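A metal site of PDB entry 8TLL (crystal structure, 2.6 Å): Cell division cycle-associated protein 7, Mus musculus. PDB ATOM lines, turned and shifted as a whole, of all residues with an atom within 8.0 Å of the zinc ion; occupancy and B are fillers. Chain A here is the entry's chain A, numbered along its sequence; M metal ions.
The guanidinium group of Arg 106 lies close to the backbone carbonyl oxygen of Cys 102. The backbone NH of Phe 104 lies close to the side-chain sulfur of Cys 102, at 3.5 Å. The side-chain hydroxyl (OH) of Tyr 78 lies close to the side-chain sulfur (SG) of Cys 100, at 3.0 Å.
Four residues have an atom within 4 Å of the zinc ion: His 44, Cys 100, Cys 102 and Cys 105. Along chain A the residues within 4 Å of the zinc ion span positions 44 to 105. The nearest printed residue that does not touch the zinc ion is Pro 95 (4.6 Å).
The zinc ion is bound by NE2 of His 44, 2.1 Å away. The zinc ion is bound by the side-chain sulfur (SG) of Cys 102 (2.3 Å). The zinc ion is bound by SG of Cys 105, at 2.3 Å. The side-chain sulfur (SG) of Cys 100 is bound to the zinc ion, at 2.3 Å. The zinc ion has four donor atoms within binding distance.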
ATOM      1  N   HIS A  44      14.322  -9.123  13.679  1.00  0.00           N
ATOM      2  CA  HIS A  44      15.684  -9.523  14.023  1.00  0.00           C
ATOM      3  C   HIS A  44      15.843  -9.751  15.520  1.00  0.00           C
ATOM      4  O   HIS A  44      16.598 -10.636  15.937  1.00  0.00           O
ATOM      5  CB  HIS A  44      16.691  -8.464  13.543  1.00  0.00           C
ATOM      6  CG  HIS A  44      18.053  -8.603  14.148  1.00  0.00           C
ATOM      7  ND1 HIS A  44      18.893  -9.661  13.877  1.00  0.00           N
ATOM      8  CD2 HIS A  44      18.738  -7.797  14.999  1.00  0.00           C
ATOM      9  CE1 HIS A  44      20.026  -9.508  14.532  1.00  0.00           C
ATOM     10  NE2 HIS A  44      19.950  -8.388  15.235  1.00  0.00           N
ATOM     11  N   GLN A  45      15.116  -8.988  16.337  1.00  0.00           N
ATOM     12  CA  GLN A  45      15.296  -9.066  17.784  1.00  0.00           C
ATOM     13  C   GLN A  45      14.616 -10.306  18.368  1.00  0.00           C
ATOM     14  O   GLN A  45      15.274 -11.169  18.937  1.00  0.00           O
ATOM     15  CB  GLN A  45      14.775  -7.776  18.440  1.00  0.00           C
ATOM     16  CG  GLN A  45      15.035  -7.683  19.935  1.00  0.00           C
ATOM     17  CD  GLN A  45      16.406  -7.103  20.271  1.00  0.00           C
ATOM     18  OE1 GLN A  45      17.048  -6.452  19.436  1.00  0.00           O
ATOM     19  NE2 GLN A  45      16.857  -7.337  21.497  1.00  0.00           N
ATOM     20  N   ARG A  47      13.022 -12.690  16.708  1.00  0.00           N
ATOM     21  CA  ARG A  47      13.150 -13.833  15.801  1.00  0.00           C
ATOM     22  C   ARG A  47      11.811 -14.560  15.620  1.00  0.00           C
ATOM     23  O   ARG A  47      11.743 -15.783  15.581  1.00  0.00           O
ATOM     24  CB  ARG A  47      14.245 -14.787  16.288  1.00  0.00           C
ATOM     25  CG  ARG A  47      15.614 -14.108  16.351  1.00  0.00           C
ATOM     26  CD  ARG A  47      16.753 -15.073  16.633  1.00  0.00           C
ATOM     27  NE  ARG A  47      16.679 -15.691  17.950  1.00  0.00           N
ATOM     28  CZ  ARG A  47      17.262 -15.223  19.036  1.00  0.00           C
ATOM     29  NH1 ARG A  47      17.951 -14.083  19.016  1.00  0.00           N
ATOM     30  NH2 ARG A  47      17.160 -15.890  20.182  1.00  0.00           N
ATOM     31  N   ARG A  66      18.398  -8.156   9.144  1.00  0.00           N
ATOM     32  CA  ARG A  66      18.782  -7.588  10.424  1.00  0.00           C
ATOM     33  C   ARG A  66      18.244  -6.177  10.649  1.00  0.00           C
ATOM     34  O   ARG A  66      18.350  -5.676  11.773  1.00  0.00           O
ATOM     35  CB  ARG A  66      20.302  -7.584  10.556  1.00  0.00           C
ATOM     36  CG  ARG A  66      21.021  -7.268   9.254  1.00  0.00           C
ATOM     37  CD  ARG A  66      22.504  -7.118   9.487  1.00  0.00           C
ATOM     38  NE  ARG A  66      22.911  -5.720   9.420  1.00  0.00           N
ATOM     39  CZ  ARG A  66      24.114  -5.273   9.762  1.00  0.00           C
ATOM     40  NH1 ARG A  66      25.043  -6.094  10.232  1.00  0.00           N
ATOM     41  NH2 ARG A  66      24.380  -3.986   9.629  1.00  0.00           N
ATOM     42  N   PHE A  69      12.530  -4.929  12.590  1.00  0.00           N
ATOM     43  CA  PHE A  69      12.180  -5.016  13.999  1.00  0.00           C
ATOM     44  C   PHE A  69      10.675  -4.860  14.141  1.00  0.00           C
ATOM     45  O   PHE A  69      10.065  -4.022  13.466  1.00  0.00           O
ATOM     46  CB  PHE A  69      12.901  -3.937  14.819  1.00  0.00           C
ATOM     47  CG  PHE A  69      14.369  -4.207  14.999  1.00  0.00           C
ATOM     48  CD1 PHE A  69      15.274  -3.921  13.994  1.00  0.00           C
ATOM     49  CD2 PHE A  69      14.837  -4.752  16.186  1.00  0.00           C
ATOM     50  CE1 PHE A  69      16.620  -4.164  14.162  1.00  0.00           C
ATOM     51  CE2 PHE A  69      16.188  -4.999  16.366  1.00  0.00           C
ATOM     52  CZ  PHE A  69      17.073  -4.710  15.348  1.00  0.00           C
ATOM     53  N   TYR A  78      14.937  -0.638  22.470  1.00  0.00           N
ATOM     54  CA  TYR A  78      15.649   0.535  21.983  1.00  0.00           C
ATOM     55  C   TYR A  78      14.920   1.857  22.206  1.00  0.00           C
ATOM     56  O   TYR A  78      15.473   2.895  21.842  1.00  0.00           O
ATOM     57  CB  TYR A  78      15.959   0.380  20.477  1.00  0.00           C
ATOM     58  CG  TYR A  78      16.679  -0.902  20.171  1.00  0.00           C
ATOM     59  CD1 TYR A  78      18.054  -1.004  20.348  1.00  0.00           C
ATOM     60  CD2 TYR A  78      15.986  -2.019  19.726  1.00  0.00           C
ATOM     61  CE1 TYR A  78      18.720  -2.192  20.071  1.00  0.00           C
ATOM     62  CE2 TYR A  78      16.638  -3.208  19.448  1.00  0.00           C
ATOM     63  CZ  TYR A  78      18.003  -3.282  19.629  1.00  0.00           C
ATOM     64  OH  TYR A  78      18.661  -4.459  19.352  1.00  0.00           O
ATOM     65  N   PRO A  94      19.589  -0.805  14.585  1.00  0.00           N
ATOM     66  CA  PRO A  94      20.535  -0.920  15.692  1.00  0.00           C
ATOM     67  C   PRO A  94      21.776  -1.724  15.322  1.00  0.00           C
ATOM     68  O   PRO A  94      22.877  -1.391  15.782  1.00  0.00           O
ATOM     69  CB  PRO A  94      19.713  -1.625  16.782  1.00  0.00           C
ATOM     70  CG  PRO A  94      18.316  -1.227  16.504  1.00  0.00           C
ATOM     71  CD  PRO A  94      18.200  -1.082  15.012  1.00  0.00           C
ATOM     72  N   PRO A  95      21.667  -2.800  14.513  1.00  0.00           N
ATOM     73  CA  PRO A  95      22.904  -3.433  14.038  1.00  0.00           C
ATOM     74  C   PRO A  95      23.827  -2.487  13.283  1.00  0.00           C
ATOM     75  O   PRO A  95      25.040  -2.545  13.471  1.00  0.00           O
ATOM     76  CB  PRO A  95      22.379  -4.554  13.140  1.00  0.00           C
ATOM     77  CG  PRO A  95      21.107  -4.934  13.765  1.00  0.00           C
ATOM     78  CD  PRO A  95      20.499  -3.649  14.227  1.00  0.00           C
ATOM     79  N   ILE A  99      24.369  -1.031  18.192  1.00  0.00           N
ATOM     80  CA  ILE A  99      23.781  -0.910  19.518  1.00  0.00           C
ATOM     81  C   ILE A  99      22.783  -2.033  19.756  1.00  0.00           C
ATOM     82  O   ILE A  99      21.984  -1.992  20.701  1.00  0.00           O
ATOM     83  CB  ILE A  99      23.113   0.469  19.719  1.00  0.00           C
ATOM     84  CG1 ILE A  99      22.032   0.693  18.661  1.00  0.00           C
ATOM     85  CG2 ILE A  99      24.157   1.586  19.660  1.00  0.00           C
ATOM     86  CD1 ILE A  99      21.254   1.976  18.833  1.00  0.00           C
ATOM     87  N   CYS A 100      22.817  -3.057  18.898  1.00  0.00           N
ATOM     88  CA  CYS A 100      21.842  -4.130  19.015  1.00  0.00           C
ATOM     89  C   CYS A 100      22.121  -4.956  20.259  1.00  0.00           C
ATOM     90  O   CYS A 100      23.258  -5.365  20.511  1.00  0.00           O
ATOM     91  CB  CYS A 100      21.868  -5.023  17.773  1.00  0.00           C
ATOM     92  SG  CYS A 100      20.523  -6.229  17.714  1.00  0.00           S
ATOM     93  N   ASN A 101      21.075  -5.184  21.058  1.00  0.00           N
ATOM     94  CA  ASN A 101      21.180  -5.952  22.284  1.00  0.00           C
ATOM     95  C   ASN A 101      20.425  -7.275  22.205  1.00  0.00           C
ATOM     96  O   ASN A 101      19.966  -7.802  23.227  1.00  0.00           O
ATOM     97  CB  ASN A 101      20.687  -5.127  23.473  1.00  0.00           C
ATOM     98  CG  ASN A 101      19.263  -4.612  23.291  1.00  0.00           C
ATOM     99  OD1 ASN A 101      18.345  -5.382  23.008  1.00  0.00           O
ATOM    100  ND2 ASN A 101      19.091  -3.313  23.455  1.00  0.00           N
ATOM    101  N   CYS A 102      20.296  -7.832  21.003  1.00  0.00           N
ATOM    102  CA  CYS A 102      19.658  -9.130  20.872  1.00  0.00           C
ATOM    103  C   CYS A 102      20.550 -10.219  21.448  1.00  0.00           C
ATOM    104  O   CYS A 102      21.722  -9.992  21.794  1.00  0.00           O
ATOM    105  CB  CYS A 102      19.311  -9.410  19.409  1.00  0.00           C
ATOM    106  SG  CYS A 102      20.663 -10.024  18.360  1.00  0.00           S
ATOM    107  N   SER A 103      19.993 -11.425  21.563  1.00  0.00           N
ATOM    108  CA  SER A 103      20.713 -12.545  22.168  1.00  0.00           C
ATOM    109  C   SER A 103      22.044 -12.783  21.487  1.00  0.00           C
ATOM    110  O   SER A 103      23.050 -13.055  22.136  1.00  0.00           O
ATOM    111  CB  SER A 103      19.864 -13.810  22.119  1.00  0.00           C
ATOM    112  OG  SER A 103      18.520 -13.552  22.486  1.00  0.00           O
ATOM    113  N   PHE A 104      22.058 -12.683  20.153  1.00  0.00           N
ATOM    114  CA  PHE A 104      23.291 -12.943  19.410  1.00  0.00           C
ATOM    115  C   PHE A 104      24.205 -11.722  19.413  1.00  0.00           C
ATOM    116  O   PHE A 104      25.390 -11.834  19.715  1.00  0.00           O
ATOM    117  CB  PHE A 104      22.939 -13.371  17.982  1.00  0.00           C
ATOM    118  CG  PHE A 104      24.125 -13.468  17.071  1.00  0.00           C
ATOM    119  CD1 PHE A 104      24.934 -14.588  17.076  1.00  0.00           C
ATOM    120  CD2 PHE A 104      24.430 -12.424  16.205  1.00  0.00           C
ATOM    121  CE1 PHE A 104      26.025 -14.660  16.236  1.00  0.00           C
ATOM    122  CE2 PHE A 104      25.521 -12.496  15.366  1.00  0.00           C
ATOM    123  CZ  PHE A 104      26.323 -13.620  15.381  1.00  0.00           C
ATOM    124  N   CYS A 105      23.659 -10.547  19.087  1.00  0.00           N
ATOM    125  CA  CYS A 105      24.494  -9.372  18.855  1.00  0.00           C
ATOM    126  C   CYS A 105      25.250  -8.953  20.110  1.00  0.00           C
ATOM    127  O   CYS A 105      26.416  -8.555  20.025  1.00  0.00           O
ATOM    128  CB  CYS A 105      23.651  -8.221  18.313  1.00  0.00           C
ATOM    129  SG  CYS A 105      23.355  -8.308  16.536  1.00  0.00           S
ATOM    130  N   ARG A 106      24.602  -9.015  21.268  1.00  0.00           N
ATOM    131  CA  ARG A 106      25.289  -8.586  22.487  1.00  0.00           C
ATOM    132  C   ARG A 106      26.349  -9.584  22.946  1.00  0.00           C
ATOM    133  O   ARG A 106      27.102  -9.259  23.882  1.00  0.00           O
ATOM    134  CB  ARG A 106      24.289  -8.326  23.602  1.00  0.00           C
ATOM    135  CG  ARG A 106      23.671  -9.564  24.204  1.00  0.00           C
ATOM    136  CD  ARG A 106      22.731  -9.161  25.314  1.00  0.00           C
ATOM    137  NE  ARG A 106      21.949 -10.287  25.817  1.00  0.00           N
ATOM    138  CZ  ARG A 106      20.697 -10.545  25.446  1.00  0.00           C
ATOM    139  NH1 ARG A 106      20.065  -9.782  24.566  1.00  0.00           N
ATOM    140  NH2 ARG A 106      20.069 -11.588  25.976  1.00  0.00           N
ATOM    141  N   GLN A 107      26.420 -10.761  22.336  1.00  0.00           N
ATOM    142  CA  GLN A 107      27.487 -11.708  22.611  1.00  0.00           C
ATOM    143  C   GLN A 107      28.629 -11.610  21.613  1.00  0.00           C
ATOM    144  O   GLN A 107      29.803 -11.636  22.018  1.00  0.00           O
ATOM    145  CB  GLN A 107      26.947 -13.143  22.612  1.00  0.00           C
ATOM    146  CG  GLN A 107      25.905 -13.416  23.690  1.00  0.00           C
ATOM    147  CD  GLN A 107      25.415 -14.843  23.684  1.00  0.00           C
ATOM    148  OE1 GLN A 107      26.201 -15.793  23.634  1.00  0.00           O
ATOM    149  NE2 GLN A 107      24.092 -15.017  23.723  1.00  0.00           N
HETATM  150 ZN    ZN M   1      21.111  -8.310  16.933  1.00  0.00          ZN
